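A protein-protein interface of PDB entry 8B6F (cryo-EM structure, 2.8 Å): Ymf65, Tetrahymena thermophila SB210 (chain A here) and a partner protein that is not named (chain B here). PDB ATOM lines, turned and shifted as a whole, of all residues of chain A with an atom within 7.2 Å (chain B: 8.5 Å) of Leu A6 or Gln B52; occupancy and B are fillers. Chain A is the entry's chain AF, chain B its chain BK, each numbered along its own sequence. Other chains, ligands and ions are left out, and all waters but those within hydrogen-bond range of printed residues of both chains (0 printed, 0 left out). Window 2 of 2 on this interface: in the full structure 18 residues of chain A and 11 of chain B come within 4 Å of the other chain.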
ATOM      1  N   ARG A   4     -17.934 -32.599 -13.798  1.00  0.00           N
ATOM      2  CA  ARG A   4     -17.775 -32.968 -12.400  1.00  0.00           C
ATOM      3  C   ARG A   4     -19.127 -32.900 -11.708  1.00  0.00           C
ATOM      4  O   ARG A   4     -19.856 -31.913 -11.859  1.00  0.00           O
ATOM      5  CB  ARG A   4     -16.773 -32.040 -11.710  1.00  0.00           C
ATOM      6  CG  ARG A   4     -16.246 -32.560 -10.388  1.00  0.00           C
ATOM      7  CD  ARG A   4     -15.178 -31.630  -9.843  1.00  0.00           C
ATOM      8  NE  ARG A   4     -14.437 -32.228  -8.740  1.00  0.00           N
ATOM      9  CZ  ARG A   4     -13.406 -31.656  -8.135  1.00  0.00           C
ATOM     10  NH1 ARG A   4     -12.968 -30.461  -8.494  1.00  0.00           N
ATOM     11  NH2 ARG A   4     -12.798 -32.300  -7.141  1.00  0.00           N
ATOM     12  N   LEU A   5     -19.460 -33.945 -10.957  1.00  0.00           N
ATOM     13  CA  LEU A   5     -20.709 -34.023 -10.207  1.00  0.00           C
ATOM     14  C   LEU A   5     -20.370 -33.844  -8.731  1.00  0.00           C
ATOM     15  O   LEU A   5     -19.906 -34.779  -8.073  1.00  0.00           O
ATOM     16  CB  LEU A   5     -21.419 -35.348 -10.463  1.00  0.00           C
ATOM     17  CG  LEU A   5     -22.757 -35.520  -9.742  1.00  0.00           C
ATOM     18  CD1 LEU A   5     -23.781 -34.510 -10.238  1.00  0.00           C
ATOM     19  CD2 LEU A   5     -23.275 -36.932  -9.908  1.00  0.00           C
ATOM     20  N   LEU A   6     -20.607 -32.644  -8.214  1.00  0.00           N
ATOM     21  CA  LEU A   6     -20.256 -32.335  -6.837  1.00  0.00           C
ATOM     22  C   LEU A   6     -21.141 -33.105  -5.864  1.00  0.00           C
ATOM     23  O   LEU A   6     -22.325 -33.330  -6.122  1.00  0.00           O
ATOM     24  CB  LEU A   6     -20.385 -30.835  -6.585  1.00  0.00           C
ATOM     25  CG  LEU A   6     -19.659 -29.925  -7.579  1.00  0.00           C
ATOM     26  CD1 LEU A   6     -19.784 -28.475  -7.151  1.00  0.00           C
ATOM     27  CD2 LEU A   6     -18.201 -30.319  -7.723  1.00  0.00           C
ATOM     28  N   VAL A   7     -20.554 -33.508  -4.734  1.00  0.00           N
ATOM     29  CA  VAL A   7     -21.324 -34.180  -3.695  1.00  0.00           C
ATOM     30  C   VAL A   7     -22.303 -33.227  -3.029  1.00  0.00           C
ATOM     31  O   VAL A   7     -23.253 -33.675  -2.377  1.00  0.00           O
ATOM     32  CB  VAL A   7     -20.372 -34.809  -2.658  1.00  0.00           C
ATOM     33  CG1 VAL A   7     -21.142 -35.379  -1.470  1.00  0.00           C
ATOM     34  CG2 VAL A   7     -19.538 -35.893  -3.302  1.00  0.00           C
ATOM     35  N   SER A   8     -22.112 -31.917  -3.188  1.00  0.00           N
ATOM     36  CA  SER A   8     -23.035 -30.962  -2.590  1.00  0.00           C
ATOM     37  C   SER A   8     -24.410 -31.028  -3.240  1.00  0.00           C
ATOM     38  O   SER A   8     -25.413 -30.696  -2.599  1.00  0.00           O
ATOM     39  CB  SER A   8     -22.465 -29.549  -2.694  1.00  0.00           C
ATOM     40  OG  SER A   8     -22.187 -29.211  -4.042  1.00  0.00           O
ATOM     41  N   GLU A   9     -24.479 -31.452  -4.504  1.00  0.00           N
ATOM     42  CA  GLU A   9     -25.755 -31.501  -5.206  1.00  0.00           C
ATOM     43  C   GLU A   9     -26.663 -32.614  -4.700  1.00  0.00           C
ATOM     44  O   GLU A   9     -27.882 -32.521  -4.871  1.00  0.00           O
ATOM     45  CB  GLU A   9     -25.519 -31.685  -6.707  1.00  0.00           C
ATOM     46  CG  GLU A   9     -24.718 -30.568  -7.359  1.00  0.00           C
ATOM     47  CD  GLU A   9     -25.484 -29.260  -7.434  1.00  0.00           C
ATOM     48  OE1 GLU A   9     -26.691 -29.255  -7.117  1.00  0.00           O
ATOM     49  OE2 GLU A   9     -24.880 -28.235  -7.814  1.00  0.00           O
ATOM     50  N   TYR A  10     -26.105 -33.665  -4.091  1.00  0.00           N
ATOM     51  CA  TYR A  10     -26.916 -34.811  -3.693  1.00  0.00           C
ATOM     52  C   TYR A  10     -26.540 -35.366  -2.323  1.00  0.00           C
ATOM     53  O   TYR A  10     -26.885 -36.513  -2.019  1.00  0.00           O
ATOM     54  CB  TYR A  10     -26.806 -35.926  -4.737  1.00  0.00           C
ATOM     55  CG  TYR A  10     -25.393 -36.407  -4.967  1.00  0.00           C
ATOM     56  CD1 TYR A  10     -24.862 -37.449  -4.220  1.00  0.00           C
ATOM     57  CD2 TYR A  10     -24.595 -35.822  -5.937  1.00  0.00           C
ATOM     58  CE1 TYR A  10     -23.570 -37.892  -4.431  1.00  0.00           C
ATOM     59  CE2 TYR A  10     -23.306 -36.256  -6.156  1.00  0.00           C
ATOM     60  CZ  TYR A  10     -22.798 -37.291  -5.402  1.00  0.00           C
ATOM     61  OH  TYR A  10     -21.513 -37.723  -5.623  1.00  0.00           O
ATOM     62  N   ILE A  11     -25.840 -34.598  -1.489  1.00  0.00           N
ATOM     63  CA  ILE A  11     -25.517 -35.083  -0.150  1.00  0.00           C
ATOM     64  C   ILE A  11     -26.788 -35.354   0.647  1.00  0.00           C
ATOM     65  O   ILE A  11     -26.892 -36.366   1.350  1.00  0.00           O
ATOM     66  CB  ILE A  11     -24.588 -34.084   0.570  1.00  0.00           C
ATOM     67  CG1 ILE A  11     -24.089 -34.661   1.898  1.00  0.00           C
ATOM     68  CG2 ILE A  11     -25.288 -32.755   0.814  1.00  0.00           C
ATOM     69  CD1 ILE A  11     -23.204 -35.883   1.755  1.00  0.00           C
ATOM     70  N   THR A  83     -28.985 -23.623  -2.618  1.00  0.00           N
ATOM     71  CA  THR A  83     -29.819 -24.598  -3.302  1.00  0.00           C
ATOM     72  C   THR A  83     -28.951 -25.707  -3.878  1.00  0.00           C
ATOM     73  O   THR A  83     -27.777 -25.499  -4.189  1.00  0.00           O
ATOM     74  CB  THR A  83     -30.625 -23.941  -4.424  1.00  0.00           C
ATOM     75  OG1 THR A  83     -29.740 -23.474  -5.449  1.00  0.00           O
ATOM     76  CG2 THR A  83     -31.437 -22.775  -3.892  1.00  0.00           C
ATOM     77  N   TRP A  85     -28.985 -29.517  -6.431  1.00  0.00           N
ATOM     78  CA  TRP A  85     -29.611 -30.289  -7.504  1.00  0.00           C
ATOM     79  C   TRP A  85     -30.407 -29.388  -8.451  1.00  0.00           C
ATOM     80  O   TRP A  85     -31.629 -29.483  -8.569  1.00  0.00           O
ATOM     81  CB  TRP A  85     -30.495 -31.401  -6.934  1.00  0.00           C
ATOM     82  CG  TRP A  85     -30.817 -32.439  -7.955  1.00  0.00           C
ATOM     83  CD1 TRP A  85     -32.026 -32.673  -8.536  1.00  0.00           C
ATOM     84  CD2 TRP A  85     -29.903 -33.376  -8.536  1.00  0.00           C
ATOM     85  NE1 TRP A  85     -31.924 -33.705  -9.438  1.00  0.00           N
ATOM     86  CE2 TRP A  85     -30.630 -34.153  -9.455  1.00  0.00           C
ATOM     87  CE3 TRP A  85     -28.540 -33.634  -8.362  1.00  0.00           C
ATOM     88  CZ2 TRP A  85     -30.041 -35.174 -10.196  1.00  0.00           C
ATOM     89  CZ3 TRP A  85     -27.955 -34.647  -9.100  1.00  0.00           C
ATOM     90  CH2 TRP A  85     -28.706 -35.404 -10.007  1.00  0.00           C
ATOM     91  N   TRP A  86     -29.679 -28.503  -9.133  1.00  0.00           N
ATOM     92  CA  TRP A  86     -30.236 -27.666 -10.192  1.00  0.00           C
ATOM     93  C   TRP A  86     -31.196 -26.616  -9.649  1.00  0.00           C
ATOM     94  O   TRP A  86     -32.152 -26.231 -10.325  1.00  0.00           O
ATOM     95  CB  TRP A  86     -30.937 -28.512 -11.260  1.00  0.00           C
ATOM     96  CG  TRP A  86     -30.132 -29.688 -11.701  1.00  0.00           C
ATOM     97  CD1 TRP A  86     -30.312 -30.987 -11.332  1.00  0.00           C
ATOM     98  CD2 TRP A  86     -29.008 -29.674 -12.587  1.00  0.00           C
ATOM     99  NE1 TRP A  86     -29.373 -31.784 -11.937  1.00  0.00           N
ATOM    100  CE2 TRP A  86     -28.559 -31.002 -12.710  1.00  0.00           C
ATOM    101  CE3 TRP A  86     -28.338 -28.666 -13.287  1.00  0.00           C
ATOM    102  CZ2 TRP A  86     -27.474 -31.352 -13.508  1.00  0.00           C
ATOM    103  CZ3 TRP A  86     -27.260 -29.014 -14.079  1.00  0.00           C
ATOM    104  CH2 TRP A  86     -26.838 -30.347 -14.184  1.00  0.00           C
ATOM    105  N   LYS B  47     -28.706 -18.936  -8.093  1.00  0.00           N
ATOM    106  CA  LYS B  47     -27.549 -19.205  -8.932  1.00  0.00           C
ATOM    107  C   LYS B  47     -28.022 -19.702 -10.288  1.00  0.00           C
ATOM    108  O   LYS B  47     -29.172 -20.117 -10.453  1.00  0.00           O
ATOM    109  CB  LYS B  47     -26.617 -20.231  -8.277  1.00  0.00           C
ATOM    110  CG  LYS B  47     -27.328 -21.510  -7.854  1.00  0.00           C
ATOM    111  CD  LYS B  47     -26.426 -22.417  -7.033  1.00  0.00           C
ATOM    112  CE  LYS B  47     -25.323 -23.031  -7.870  1.00  0.00           C
ATOM    113  NZ  LYS B  47     -25.857 -23.901  -8.954  1.00  0.00           N
ATOM    114  N   LEU B  48     -27.115 -19.652 -11.259  1.00  0.00           N
ATOM    115  CA  LEU B  48     -27.380 -20.223 -12.565  1.00  0.00           C
ATOM    116  C   LEU B  48     -27.370 -21.746 -12.473  1.00  0.00           C
ATOM    117  O   LEU B  48     -26.806 -22.317 -11.538  1.00  0.00           O
ATOM    118  CB  LEU B  48     -26.342 -19.750 -13.579  1.00  0.00           C
ATOM    119  CG  LEU B  48     -26.406 -18.279 -13.996  1.00  0.00           C
ATOM    120  CD1 LEU B  48     -25.716 -17.389 -12.975  1.00  0.00           C
ATOM    121  CD2 LEU B  48     -25.791 -18.087 -15.371  1.00  0.00           C
ATOM    122  N   PRO B  49     -27.998 -22.432 -13.432  1.00  0.00           N
ATOM    123  CA  PRO B  49     -28.057 -23.902 -13.340  1.00  0.00           C
ATOM    124  C   PRO B  49     -26.692 -24.561 -13.243  1.00  0.00           C
ATOM    125  O   PRO B  49     -26.539 -25.541 -12.505  1.00  0.00           O
ATOM    126  CB  PRO B  49     -28.799 -24.303 -14.626  1.00  0.00           C
ATOM    127  CG  PRO B  49     -28.709 -23.114 -15.526  1.00  0.00           C
ATOM    128  CD  PRO B  49     -28.699 -21.928 -14.624  1.00  0.00           C
ATOM    129  N   GLY B  50     -25.696 -24.055 -13.962  1.00  0.00           N
ATOM    130  CA  GLY B  50     -24.367 -24.627 -13.963  1.00  0.00           C
ATOM    131  C   GLY B  50     -23.342 -23.892 -13.127  1.00  0.00           C
ATOM    132  O   GLY B  50     -22.160 -24.251 -13.175  1.00  0.00           O
ATOM    133  N   GLN B  51     -23.744 -22.881 -12.365  1.00  0.00           N
ATOM    134  CA  GLN B  51     -22.799 -22.106 -11.575  1.00  0.00           C
ATOM    135  C   GLN B  51     -22.394 -22.865 -10.318  1.00  0.00           C
ATOM    136  O   GLN B  51     -23.209 -23.554  -9.699  1.00  0.00           O
ATOM    137  CB  GLN B  51     -23.407 -20.755 -11.200  1.00  0.00           C
ATOM    138  CG  GLN B  51     -22.468 -19.846 -10.431  1.00  0.00           C
ATOM    139  CD  GLN B  51     -23.051 -18.467 -10.214  1.00  0.00           C
ATOM    140  OE1 GLN B  51     -24.237 -18.238 -10.443  1.00  0.00           O
ATOM    141  NE2 GLN B  51     -22.215 -17.535  -9.771  1.00  0.00           N
ATOM    142  N   GLN B  52     -21.123 -22.733  -9.944  1.00  0.00           N
ATOM    143  CA  GLN B  52     -20.600 -23.326  -8.723  1.00  0.00           C
ATOM    144  C   GLN B  52     -19.561 -22.381  -8.137  1.00  0.00           C
ATOM    145  O   GLN B  52     -19.001 -21.535  -8.836  1.00  0.00           O
ATOM    146  CB  GLN B  52     -19.977 -24.705  -8.977  1.00  0.00           C
ATOM    147  CG  GLN B  52     -20.940 -25.733  -9.553  1.00  0.00           C
ATOM    148  CD  GLN B  52     -22.051 -26.100  -8.591  1.00  0.00           C
ATOM    149  OE1 GLN B  52     -21.997 -25.772  -7.408  1.00  0.00           O
ATOM    150  NE2 GLN B  52     -23.067 -26.788  -9.097  1.00  0.00           N
ATOM    151  N   TYR B  53     -19.308 -22.533  -6.840  1.00  0.00           N
ATOM    152  CA  TYR B  53     -18.409 -21.652  -6.108  1.00  0.00           C
ATOM    153  C   TYR B  53     -17.198 -22.437  -5.628  1.00  0.00           C
ATOM    154  O   TYR B  53     -17.347 -23.502  -5.020  1.00  0.00           O
ATOM    155  CB  TYR B  53     -19.122 -21.009  -4.915  1.00  0.00           C
ATOM    156  CG  TYR B  53     -20.401 -20.297  -5.283  1.00  0.00           C
ATOM    157  CD1 TYR B  53     -20.374 -19.056  -5.905  1.00  0.00           C
ATOM    158  CD2 TYR B  53     -21.637 -20.865  -5.008  1.00  0.00           C
ATOM    159  CE1 TYR B  53     -21.540 -18.402  -6.243  1.00  0.00           C
ATOM    160  CE2 TYR B  53     -22.809 -20.218  -5.344  1.00  0.00           C
ATOM    161  CZ  TYR B  53     -22.754 -18.987  -5.961  1.00  0.00           C
ATOM    162  OH  TYR B  53     -23.918 -18.338  -6.296  1.00  0.00           O
ATOM    163  N   ASP B  54     -16.004 -21.909  -5.901  1.00  0.00           N
ATOM    164  CA  ASP B  54     -14.761 -22.492  -5.398  1.00  0.00           C
ATOM    165  C   ASP B  54     -14.444 -21.804  -4.078  1.00  0.00           C
ATOM    166  O   ASP B  54     -13.740 -20.796  -4.026  1.00  0.00           O
ATOM    167  CB  ASP B  54     -13.635 -22.329  -6.410  1.00  0.00           C
ATOM    168  CG  ASP B  54     -12.397 -23.114  -6.031  1.00  0.00           C
ATOM    169  OD1 ASP B  54     -12.431 -23.819  -5.001  1.00  0.00           O
ATOM    170  OD2 ASP B  54     -11.389 -23.026  -6.762  1.00  0.00           O
ATOM    171  N   TYR B  55     -14.976 -22.365  -2.992  1.00  0.00           N
ATOM    172  CA  TYR B  55     -14.897 -21.701  -1.697  1.00  0.00           C
ATOM    173  C   TYR B  55     -13.457 -21.579  -1.216  1.00  0.00           C
ATOM    174  O   TYR B  55     -13.080 -20.560  -0.629  1.00  0.00           O
ATOM    175  CB  TYR B  55     -15.743 -22.456  -0.676  1.00  0.00           C
ATOM    176  CG  TYR B  55     -17.230 -22.268  -0.873  1.00  0.00           C
ATOM    177  CD1 TYR B  55     -17.849 -21.072  -0.536  1.00  0.00           C
ATOM    178  CD2 TYR B  55     -18.014 -23.288  -1.393  1.00  0.00           C
ATOM    179  CE1 TYR B  55     -19.208 -20.897  -0.713  1.00  0.00           C
ATOM    180  CE2 TYR B  55     -19.372 -23.124  -1.575  1.00  0.00           C
ATOM    181  CZ  TYR B  55     -19.963 -21.928  -1.233  1.00  0.00           C
ATOM    182  OH  TYR B  55     -21.317 -21.764  -1.413  1.00  0.00           O
ATOM    183  N   ARG B  57     -10.645 -21.186  -2.948  1.00  0.00           N
ATOM    184  CA  ARG B  57      -9.984 -20.071  -3.615  1.00  0.00           C
ATOM    185  C   ARG B  57     -10.585 -18.738  -3.187  1.00  0.00           C
ATOM    186  O   ARG B  57      -9.853 -17.780  -2.914  1.00  0.00           O
ATOM    187  CB  ARG B  57     -10.072 -20.250  -5.128  1.00  0.00           C
ATOM    188  CG  ARG B  57      -9.284 -19.225  -5.921  1.00  0.00           C
ATOM    189  CD  ARG B  57      -9.072 -19.688  -7.353  1.00  0.00           C
ATOM    190  NE  ARG B  57     -10.330 -19.847  -8.074  1.00  0.00           N
ATOM    191  CZ  ARG B  57     -10.888 -18.922  -8.844  1.00  0.00           C
ATOM    192  NH1 ARG B  57     -10.326 -17.738  -9.024  1.00  0.00           N
ATOM    193  NH2 ARG B  57     -12.038 -19.195  -9.454  1.00  0.00           N
ATOM    194  N   SER B  92     -11.853 -14.064  -7.649  1.00  0.00           N
ATOM    195  CA  SER B  92     -12.071 -15.347  -6.990  1.00  0.00           C
ATOM    196  C   SER B  92     -13.474 -15.475  -6.413  1.00  0.00           C
ATOM    197  O   SER B  92     -14.094 -16.537  -6.527  1.00  0.00           O
ATOM    198  CB  SER B  92     -11.034 -15.543  -5.885  1.00  0.00           C
ATOM    199  OG  SER B  92      -9.721 -15.532  -6.417  1.00  0.00           O
ATOM    200  N   ASP B  94     -17.592 -14.509  -5.633  1.00  0.00           N
ATOM    201  CA  ASP B  94     -18.802 -14.113  -6.331  1.00  0.00           C
ATOM    202  C   ASP B  94     -19.386 -12.844  -5.715  1.00  0.00           C
ATOM    203  O   ASP B  94     -19.049 -12.449  -4.597  1.00  0.00           O
ATOM    204  CB  ASP B  94     -19.830 -15.245  -6.286  1.00  0.00           C
ATOM    205  CG  ASP B  94     -21.008 -15.004  -7.208  1.00  0.00           C
ATOM    206  OD1 ASP B  94     -20.812 -15.006  -8.440  1.00  0.00           O
ATOM    207  OD2 ASP B  94     -22.132 -14.816  -6.699  1.00  0.00           O
ATOM    208  N   ILE B  97     -21.225 -13.424  -2.380  1.00  0.00           N
ATOM    209  CA  ILE B  97     -20.277 -13.675  -1.299  1.00  0.00           C
ATOM    210  C   ILE B  97     -19.601 -12.377  -0.880  1.00  0.00           C
ATOM    211  O   ILE B  97     -19.435 -12.102   0.314  1.00  0.00           O
ATOM    212  CB  ILE B  97     -19.252 -14.742  -1.727  1.00  0.00           C
ATOM    213  CG1 ILE B  97     -19.957 -16.081  -1.954  1.00  0.00           C
ATOM    214  CG2 ILE B  97     -18.141 -14.875  -0.685  1.00  0.00           C
ATOM    215  CD1 ILE B  97     -19.086 -17.141  -2.581  1.00  0.00           C
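OE2 of Glu A9 lies within hydrogen-bond range of NE2 of Gln B52, 2.7 Å away.
The side-chain amino group (NZ) of Lys B47 lies within hydrogen-bond range of the backbone carbonyl oxygen (O) of Gln B51, at 2.8 Å.
The side-chain carboxylate (OE1) of Glu A9 is in hydrogen-bond range of the backbone NH (N) of Trp A85 (2.4 Å).
Among the printed residues, merely in contact across the chains: Leu A6 with Gln B52 (3.5 Å), Trp A86 with Pro B49 (3.7 Å) and Thr A83 with Lys B47 (3.8 Å).
Leu A5 touches none of the printed residues of chain B.
Leu A6 touches just one residue of chain B: Gln B52 (3.5 Å).
Printed residues of chain B within 4 Å of Glu A9: Gln B52 (2.7 Å).
Of the printed residues of chain B, Thr A83 touches Lys B47 (3.8 Å).
Of the printed residues of chain B, Trp A86 touches Pro B49.
Printed residues of chain A within 4 Å of Lys B47: Thr A83 (3.8 Å).
Of the printed residues of chain A, Pro B49 touches Trp A86.
Of chain A, only Leu A6 (3.5 Å) and Glu A9 (2.7 Å) come within 4 Å of Gln B52.
Ile B97 touches none of the printed residues of chain A.
The nearest residue of chain B that does not touch Leu A6 is Tyr B53 (5.9 Å).
The nearest residue of chain A that does not touch Gln B52 is Ser A8 (4.8 Å).
Printed residues of chain A that touch a printed residue of chain B: Leu A6, Glu A9, Thr A83 and Trp A86.
Of the 13 printed residues of chain B, 3 touch a printed residue of chain A.
Printed residues of chain B that touch a printed residue of chain A: Lys B47, Pro B49 and Gln B52.
Among the printed residues, 4 pairs touch across the chains.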
